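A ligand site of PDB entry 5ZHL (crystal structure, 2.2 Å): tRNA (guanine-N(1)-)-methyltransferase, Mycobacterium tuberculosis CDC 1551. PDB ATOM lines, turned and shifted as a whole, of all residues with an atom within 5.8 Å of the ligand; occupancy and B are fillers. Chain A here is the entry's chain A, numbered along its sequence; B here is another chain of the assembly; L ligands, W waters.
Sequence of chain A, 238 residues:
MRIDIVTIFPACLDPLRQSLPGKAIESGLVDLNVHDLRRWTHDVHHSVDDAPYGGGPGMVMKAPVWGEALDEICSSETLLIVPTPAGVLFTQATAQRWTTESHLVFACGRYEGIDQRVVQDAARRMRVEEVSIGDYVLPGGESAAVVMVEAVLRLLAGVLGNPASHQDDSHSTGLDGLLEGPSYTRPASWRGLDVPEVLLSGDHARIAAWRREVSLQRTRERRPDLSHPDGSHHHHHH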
ATOM      1  N   PRO A  57      15.498   9.944  26.441  1.00  0.00           N
ATOM      2  CA  PRO A  57      16.674  10.413  27.188  1.00  0.00           C
ATOM      3  C   PRO A  57      16.825  11.929  27.069  1.00  0.00           C
ATOM      4  O   PRO A  57      16.360  12.525  26.090  1.00  0.00           O
ATOM      5  CB  PRO A  57      17.828   9.671  26.524  1.00  0.00           C
ATOM      6  CG  PRO A  57      17.379   9.465  25.098  1.00  0.00           C
ATOM      7  CD  PRO A  57      15.866   9.466  25.093  1.00  0.00           C
ATOM      8  N   GLY A  58      17.454  12.516  28.063  1.00  0.00           N
ATOM      9  CA  GLY A  58      17.788  13.936  28.112  1.00  0.00           C
ATOM     10  C   GLY A  58      16.659  14.942  28.034  1.00  0.00           C
ATOM     11  O   GLY A  58      15.531  14.699  28.472  1.00  0.00           O
ATOM     12  N   PRO A  83      21.889  23.195  12.256  1.00  0.00           N
ATOM     13  CA  PRO A  83      22.803  22.046  12.267  1.00  0.00           C
ATOM     14  C   PRO A  83      22.132  20.924  13.081  1.00  0.00           C
ATOM     15  O   PRO A  83      21.648  21.163  14.186  1.00  0.00           O
ATOM     16  CB  PRO A  83      24.044  22.585  12.938  1.00  0.00           C
ATOM     17  CG  PRO A  83      23.894  24.131  12.856  1.00  0.00           C
ATOM     18  CD  PRO A  83      22.420  24.302  13.051  1.00  0.00           C
ATOM     19  N   THR A  84      22.048  19.724  12.491  1.00  0.00           N
ATOM     20  CA  THR A  84      21.391  18.591  13.156  1.00  0.00           C
ATOM     21  C   THR A  84      21.922  17.276  12.636  1.00  0.00           C
ATOM     22  O   THR A  84      22.155  17.163  11.442  1.00  0.00           O
ATOM     23  CB  THR A  84      19.806  18.659  13.052  1.00  0.00           C
ATOM     24  OG1 THR A  84      19.279  17.370  13.266  1.00  0.00           O
ATOM     25  CG2 THR A  84      19.293  19.144  11.721  1.00  0.00           C
ATOM     26  N   PRO A  85      22.043  16.239  13.483  1.00  0.00           N
ATOM     27  CA  PRO A  85      22.470  14.925  12.967  1.00  0.00           C
ATOM     28  C   PRO A  85      21.430  14.266  12.033  1.00  0.00           C
ATOM     29  O   PRO A  85      21.739  13.319  11.337  1.00  0.00           O
ATOM     30  CB  PRO A  85      22.681  14.105  14.246  1.00  0.00           C
ATOM     31  CG  PRO A  85      21.699  14.697  15.232  1.00  0.00           C
ATOM     32  CD  PRO A  85      21.755  16.187  14.941  1.00  0.00           C
ATOM     33  N   GLY A 109      21.899  23.858  18.384  1.00  0.00           N
ATOM     34  CA  GLY A 109      21.246  23.124  19.453  1.00  0.00           C
ATOM     35  C   GLY A 109      22.200  22.395  20.368  1.00  0.00           C
ATOM     36  O   GLY A 109      23.326  22.079  19.988  1.00  0.00           O
ATOM     37  N   ARG A 110      21.743  22.164  21.606  1.00  0.00           N
ATOM     38  CA  ARG A 110      22.414  21.367  22.639  1.00  0.00           C
ATOM     39  C   ARG A 110      21.358  20.371  23.135  1.00  0.00           C
ATOM     40  O   ARG A 110      20.248  20.365  22.587  1.00  0.00           O
ATOM     41  CB  ARG A 110      22.934  22.255  23.796  1.00  0.00           C
ATOM     42  CG  ARG A 110      24.255  22.931  23.496  1.00  0.00           C
ATOM     43  CD  ARG A 110      25.442  22.031  23.724  1.00  0.00           C
ATOM     44  NE  ARG A 110      26.597  22.522  22.979  1.00  0.00           N
ATOM     45  CZ  ARG A 110      27.842  22.075  23.128  1.00  0.00           C
ATOM     46  NH1 ARG A 110      28.100  21.114  24.012  1.00  0.00           N
ATOM     47  NH2 ARG A 110      28.821  22.587  22.414  1.00  0.00           N
ATOM     48  N   TYR A 111      21.670  19.567  24.180  1.00  0.00           N
ATOM     49  CA  TYR A 111      20.766  18.547  24.751  1.00  0.00           C
ATOM     50  C   TYR A 111      20.407  17.503  23.652  1.00  0.00           C
ATOM     51  O   TYR A 111      21.312  17.000  22.993  1.00  0.00           O
ATOM     52  CB  TYR A 111      19.529  19.184  25.429  1.00  0.00           C
ATOM     53  CG  TYR A 111      19.879  20.274  26.422  1.00  0.00           C
ATOM     54  CD1 TYR A 111      20.367  19.966  27.685  1.00  0.00           C
ATOM     55  CD2 TYR A 111      19.729  21.626  26.086  1.00  0.00           C
ATOM     56  CE1 TYR A 111      20.700  20.965  28.598  1.00  0.00           C
ATOM     57  CE2 TYR A 111      20.073  22.633  26.986  1.00  0.00           C
ATOM     58  CZ  TYR A 111      20.556  22.301  28.245  1.00  0.00           C
ATOM     59  OH  TYR A 111      20.882  23.297  29.136  1.00  0.00           O
ATOM     60  N   GLU A 112      19.106  17.234  23.400  1.00  0.00           N
ATOM     61  CA  GLU A 112      18.715  16.288  22.349  1.00  0.00           C
ATOM     62  C   GLU A 112      18.234  16.994  21.075  1.00  0.00           C
ATOM     63  O   GLU A 112      17.816  16.345  20.122  1.00  0.00           O
ATOM     64  CB  GLU A 112      17.687  15.255  22.872  1.00  0.00           C
ATOM     65  CG  GLU A 112      18.217  14.385  24.005  1.00  0.00           C
ATOM     66  CD  GLU A 112      19.399  13.490  23.661  1.00  0.00           C
ATOM     67  OE1 GLU A 112      19.186  12.522  22.886  1.00  0.00           O
ATOM     68  OE2 GLU A 112      20.505  13.721  24.186  1.00  0.00           O
ATOM     69  N   GLY A 113      18.366  18.308  21.059  1.00  0.00           N
ATOM     70  CA  GLY A 113      17.995  19.124  19.906  1.00  0.00           C
ATOM     71  C   GLY A 113      16.930  20.134  20.240  1.00  0.00           C
ATOM     72  O   GLY A 113      16.608  20.341  21.409  1.00  0.00           O
ATOM     73  N   VAL A 131      20.853  20.573   8.376  1.00  0.00           N
ATOM     74  CA  VAL A 131      22.129  20.095   7.835  1.00  0.00           C
ATOM     75  C   VAL A 131      23.012  19.328   8.839  1.00  0.00           C
ATOM     76  O   VAL A 131      23.268  19.782   9.957  1.00  0.00           O
ATOM     77  CB  VAL A 131      22.877  21.312   7.205  1.00  0.00           C
ATOM     78  CG1 VAL A 131      24.281  20.970   6.703  1.00  0.00           C
ATOM     79  CG2 VAL A 131      22.063  21.964   6.075  1.00  0.00           C
ATOM     80  N   SER A 132      23.555  18.205   8.372  1.00  0.00           N
ATOM     81  CA  SER A 132      24.514  17.417   9.131  1.00  0.00           C
ATOM     82  C   SER A 132      25.878  17.625   8.477  1.00  0.00           C
ATOM     83  O   SER A 132      25.930  17.759   7.261  1.00  0.00           O
ATOM     84  CB  SER A 132      24.158  15.934   9.083  1.00  0.00           C
ATOM     85  OG  SER A 132      25.155  15.220   9.776  1.00  0.00           O
ATOM     86  N   ILE A 133      26.964  17.628   9.256  1.00  0.00           N
ATOM     87  CA  ILE A 133      28.325  17.755   8.705  1.00  0.00           C
ATOM     88  C   ILE A 133      28.930  16.365   8.462  1.00  0.00           C
ATOM     89  O   ILE A 133      29.963  16.257   7.813  1.00  0.00           O
ATOM     90  CB  ILE A 133      29.270  18.709   9.462  1.00  0.00           C
ATOM     91  CG1 ILE A 133      29.398  18.337  10.968  1.00  0.00           C
ATOM     92  CG2 ILE A 133      28.888  20.167   9.249  1.00  0.00           C
ATOM     93  CD1 ILE A 133      30.715  18.718  11.632  1.00  0.00           C
ATOM     94  N   GLY A 134      28.248  15.318   8.923  1.00  0.00           N
ATOM     95  CA  GLY A 134      28.748  13.957   8.714  1.00  0.00           C
ATOM     96  C   GLY A 134      28.163  12.900   9.617  1.00  0.00           C
ATOM     97  O   GLY A 134      27.551  13.224  10.632  1.00  0.00           O
ATOM     98  N   ASP A 135      28.444  11.630   9.294  1.00  0.00           N
ATOM     99  CA  ASP A 135      27.922  10.458  10.012  1.00  0.00           C
ATOM    100  C   ASP A 135      28.657  10.121  11.323  1.00  0.00           C
ATOM    101  O   ASP A 135      29.226   9.044  11.487  1.00  0.00           O
ATOM    102  CB  ASP A 135      27.879   9.256   9.050  1.00  0.00           C
ATOM    103  CG  ASP A 135      26.869   9.487   7.939  1.00  0.00           C
ATOM    104  OD1 ASP A 135      25.921  10.273   8.147  1.00  0.00           O
ATOM    105  OD2 ASP A 135      27.007   8.855   6.866  1.00  0.00           O
ATOM    106  N   TYR A 136      28.618  11.054  12.273  1.00  0.00           N
ATOM    107  CA  TYR A 136      29.204  10.960  13.613  1.00  0.00           C
ATOM    108  C   TYR A 136      28.374  11.825  14.528  1.00  0.00           C
ATOM    109  O   TYR A 136      27.691  12.719  14.045  1.00  0.00           O
ATOM    110  CB  TYR A 136      30.673  11.398  13.620  1.00  0.00           C
ATOM    111  CG  TYR A 136      30.975  12.558  12.713  1.00  0.00           C
ATOM    112  CD1 TYR A 136      30.842  13.873  13.162  1.00  0.00           C
ATOM    113  CD2 TYR A 136      31.502  12.356  11.440  1.00  0.00           C
ATOM    114  CE1 TYR A 136      31.095  14.959  12.313  1.00  0.00           C
ATOM    115  CE2 TYR A 136      31.787  13.435  10.597  1.00  0.00           C
ATOM    116  CZ  TYR A 136      31.589  14.729  11.040  1.00  0.00           C
ATOM    117  OH  TYR A 136      31.879  15.788  10.216  1.00  0.00           O
ATOM    118  N   VAL A 137      28.411  11.554  15.830  1.00  0.00           N
ATOM    119  CA  VAL A 137      27.602  12.264  16.838  1.00  0.00           C
ATOM    120  C   VAL A 137      28.428  13.286  17.641  1.00  0.00           C
ATOM    121  O   VAL A 137      29.473  12.950  18.231  1.00  0.00           O
ATOM    122  CB  VAL A 137      26.849  11.267  17.759  1.00  0.00           C
ATOM    123  CG1 VAL A 137      25.877  11.999  18.683  1.00  0.00           C
ATOM    124  CG2 VAL A 137      26.101  10.218  16.930  1.00  0.00           C
ATOM    125  N   LEU A 138      27.958  14.549  17.648  1.00  0.00           N
ATOM    126  CA  LEU A 138      28.581  15.658  18.320  1.00  0.00           C
ATOM    127  C   LEU A 138      27.755  16.063  19.552  1.00  0.00           C
ATOM    128  O   LEU A 138      26.539  15.817  19.573  1.00  0.00           O
ATOM    129  CB  LEU A 138      28.673  16.852  17.341  1.00  0.00           C
ATOM    130  CG  LEU A 138      29.524  16.641  16.089  1.00  0.00           C
ATOM    131  CD1 LEU A 138      29.330  17.790  15.128  1.00  0.00           C
ATOM    132  CD2 LEU A 138      30.978  16.483  16.429  1.00  0.00           C
ATOM    133  N   PRO A 139      28.367  16.718  20.559  1.00  0.00           N
ATOM    134  CA  PRO A 139      27.572  17.140  21.728  1.00  0.00           C
ATOM    135  C   PRO A 139      26.644  18.328  21.451  1.00  0.00           C
ATOM    136  O   PRO A 139      25.667  18.504  22.169  1.00  0.00           O
ATOM    137  CB  PRO A 139      28.636  17.438  22.788  1.00  0.00           C
ATOM    138  CG  PRO A 139      29.835  17.837  22.010  1.00  0.00           C
ATOM    139  CD  PRO A 139      29.790  17.092  20.716  1.00  0.00           C
ATOM    140  N   GLY A 140      26.911  19.085  20.391  1.00  0.00           N
ATOM    141  CA  GLY A 140      26.083  20.224  20.010  1.00  0.00           C
ATOM    142  C   GLY A 140      26.444  20.727  18.621  1.00  0.00           C
ATOM    143  O   GLY A 140      27.370  20.202  18.007  1.00  0.00           O
ATOM    144  N   GLY A 141      25.746  21.760  18.151  1.00  0.00           N
ATOM    145  CA  GLY A 141      25.950  22.243  16.798  1.00  0.00           C
ATOM    146  C   GLY A 141      26.913  23.398  16.561  1.00  0.00           C
ATOM    147  O   GLY A 141      26.984  23.881  15.426  1.00  0.00           O
ATOM    148  N   ALA A 144      29.994  22.333  14.458  1.00  0.00           N
ATOM    149  CA  ALA A 144      29.509  22.043  13.109  1.00  0.00           C
ATOM    150  C   ALA A 144      29.287  23.400  12.402  1.00  0.00           C
ATOM    151  O   ALA A 144      29.606  23.525  11.219  1.00  0.00           O
ATOM    152  CB  ALA A 144      28.203  21.260  13.191  1.00  0.00           C
ATOM    153  N   MET A 148      31.006  24.824   8.954  1.00  0.00           N
ATOM    154  CA  MET A 148      30.189  25.363   7.852  1.00  0.00           C
ATOM    155  C   MET A 148      30.541  26.807   7.497  1.00  0.00           C
ATOM    156  O   MET A 148      30.701  27.128   6.307  1.00  0.00           O
ATOM    157  CB  MET A 148      28.705  25.191   8.156  1.00  0.00           C
ATOM    158  CG  MET A 148      28.258  23.716   8.128  1.00  0.00           C
ATOM    159  SD  MET A 148      26.441  23.560   8.299  1.00  0.00           S
ATOM    160  CE  MET A 148      26.260  23.744   9.978  1.00  0.00           C
ATOM    161  N   ARG B 154      32.842  12.800  24.118  1.00  0.00           N
ATOM    162  CA  ARG B 154      31.466  12.526  24.571  1.00  0.00           C
ATOM    163  C   ARG B 154      31.217  11.055  24.781  1.00  0.00           C
ATOM    164  O   ARG B 154      30.332  10.717  25.572  1.00  0.00           O
ATOM    165  CB  ARG B 154      30.395  13.176  23.674  1.00  0.00           C
ATOM    166  CG  ARG B 154      30.277  12.528  22.312  1.00  0.00           C
ATOM    167  CD  ARG B 154      29.070  13.024  21.553  1.00  0.00           C
ATOM    168  NE  ARG B 154      27.782  12.626  22.126  1.00  0.00           N
ATOM    169  CZ  ARG B 154      27.148  11.473  21.907  1.00  0.00           C
ATOM    170  NH1 ARG B 154      27.721  10.515  21.171  1.00  0.00           N
ATOM    171  NH2 ARG B 154      25.950  11.252  22.416  1.00  0.00           N
ATOM    172  N   GLU B 180      17.761  10.310  13.567  1.00  0.00           N
ATOM    173  CA  GLU B 180      16.952  10.662  14.740  1.00  0.00           C
ATOM    174  C   GLU B 180      15.668  11.335  14.276  1.00  0.00           C
ATOM    175  O   GLU B 180      15.677  12.073  13.285  1.00  0.00           O
ATOM    176  CB  GLU B 180      17.740  11.596  15.656  1.00  0.00           C
ATOM    177  CG  GLU B 180      18.822  10.886  16.458  1.00  0.00           C
ATOM    178  CD  GLU B 180      18.340   9.996  17.595  1.00  0.00           C
ATOM    179  OE1 GLU B 180      19.037   9.017  17.915  1.00  0.00           O
ATOM    180  OE2 GLU B 180      17.255  10.292  18.161  1.00  0.00           O
HETATM  181  C1  LIG L   1      22.682  10.076  28.772  1.00  0.00           C
HETATM  182  C2  LIG L   1      22.254  11.287  27.919  1.00  0.00           C
HETATM  183  C3  LIG L   1      21.334  10.837  26.782  1.00  0.00           C
HETATM  184  C4  LIG L   1      22.134  10.743  25.477  1.00  0.00           C
HETATM  185  C5  LIG L   1      21.220  10.314  24.329  1.00  0.00           C
HETATM  186  C6  LIG L   1      21.923  10.608  22.996  1.00  0.00           C
HETATM  187  C7  LIG L   1      21.108   9.986  21.852  1.00  0.00           C
HETATM  188  C8  LIG L   1      21.308  10.799  20.565  1.00  0.00           C
HETATM  189  N1  LIG L   1      20.422  11.969  20.518  1.00  0.00           N
HETATM  190  C9  LIG L   1      20.424  12.647  19.209  1.00  0.00           C
HETATM  191  C10 LIG L   1      21.254  13.782  19.136  1.00  0.00           C
HETATM  192  C11 LIG L   1      20.699  15.077  19.041  1.00  0.00           C
HETATM  193  C12 LIG L   1      21.525  16.210  18.895  1.00  0.00           C
HETATM  194  C13 LIG L   1      22.639  13.631  19.024  1.00  0.00           C
HETATM  195  C14 LIG L   1      23.462  14.749  18.895  1.00  0.00           C
HETATM  196  C15 LIG L   1      22.918  16.038  18.833  1.00  0.00           C
HETATM  197  C16 LIG L   1      23.772  17.148  18.667  1.00  0.00           C
HETATM  198  N2  LIG L   1      24.345  17.199  17.286  1.00  0.00           N
HETATM  199  C17 LIG L   1      24.370  18.306  16.510  1.00  0.00           C
HETATM  200  O1  LIG L   1      23.859  19.347  16.926  1.00  0.00           O
HETATM  201  C18 LIG L   1      24.887  18.254  15.221  1.00  0.00           C
HETATM  202  C19 LIG L   1      25.508  17.234  14.513  1.00  0.00           C
HETATM  203  C20 LIG L   1      25.901  15.953  14.825  1.00  0.00           C
HETATM  204  O2  LIG L   1      25.743  15.409  15.928  1.00  0.00           O
HETATM  205  N3  LIG L   1      26.500  15.122  13.864  1.00  0.00           N
HETATM  206  C21 LIG L   1      26.809  15.532  12.660  1.00  0.00           C
HETATM  207  N4  LIG L   1      26.454  16.828  12.344  1.00  0.00           N
HETATM  208  C22 LIG L   1      25.798  17.617  13.223  1.00  0.00           C
HETATM  209  S1  LIG L   1      25.332  19.162  12.912  1.00  0.00           S
HETATM  210  C23 LIG L   1      24.717  19.369  14.468  1.00  0.00           C
HETATM  211  O   HOH W   1      17.187  12.319  21.054  1.00  0.00           O
HETATM  212  O   HOH W   2      22.650  21.792  16.617  1.00  0.00           O
HETATM  213  O   HOH W   3      17.340  13.966  18.900  1.00  0.00           O
HETATM  214  O   HOH W   4      21.417  19.796  18.697  1.00  0.00           O
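The backbone NH (N) of Gly 141 is in hydrogen-bond range of an oxygen (O1) of the ligand (3.3 Å).
The side-chain carboxylate (OE1) of Glu 112 is in salt-bridge range of a nitrogen (N1) of the ligand (2.7 Å).
The backbone carbonyl oxygen (O) of Tyr 136 lies within hydrogen-bond range of a nitrogen (N3) of the ligand (2.7 Å).
The backbone NH of Thr 84 lies close to a sulfur (S1) of the ligand, 3.4 Å away.
The side-chain hydroxyl of Ser 132 sits at hydrogen-bond distance from a nitrogen (N4) of the ligand (3.3 Å).
N4 of the ligand is in hydrogen-bond range of N of Ile 133 (3.2 Å).
N of Leu 138 lies within hydrogen-bond range of O2 of the ligand, 2.9 Å away.
The backbone carbonyl oxygen (O) of Leu 138 lies close to a nitrogen (N2) of the ligand, 3.5 Å away.
The backbone NH (N) of Gly 134 sits at hydrogen-bond distance from the side-chain hydroxyl (OG) of Ser 132 (3.2 Å).
The backbone carbonyl oxygen (O) of Ile 133 is in hydrogen-bond range of the side-chain hydroxyl (OH) of Tyr 136, 3.1 Å away.
The backbone carbonyl oxygen (O) of Gly 109 sits at hydrogen-bond distance from the backbone NH (N) of Gly 141 (3.1 Å).
The backbone NH (N) of Thr 84 sits at hydrogen-bond distance from the backbone carbonyl oxygen (O) of Val 131 (2.8 Å).
S1 of the ligand lies close to O of Val 131 (3.7 Å).
Merely in contact with the ligand: Pro 57, Pro 83, Pro 85, Gly 134, Val 137, Gly 140, Ala 144 and Glu 180 of chain B.
16 residues have an atom within 4 Å of the ligand: Pro 57, Pro 83, Thr 84, Pro 85, Glu 112, Val 131, Ser 132, Ile 133, Gly 134, Tyr 136, Val 137, Leu 138, Gly 140, Gly 141, Ala 144 and Glu 180 of chain B.
The nearest printed residue that does not touch the ligand is Arg 154 of chain B (4.1 Å).
Water W2 lies within hydrogen-bond range of the backbone carbonyl oxygen (O) of Pro 83 (2.7 Å), an oxygen (O1) of the ligand (2.7 Å), the backbone NH (N) of Gly 109 (2.8 Å) and the backbone NH (N) of Gly 141 (3.5 Å).
Water W4 bridges O1 of the ligand (3.0 Å) and O of Gly 109 (3.2 Å).
Water W1 lies within hydrogen-bond range of OE1 of Glu 112 (2.7 Å) and N1 of the ligand (3.3 Å).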
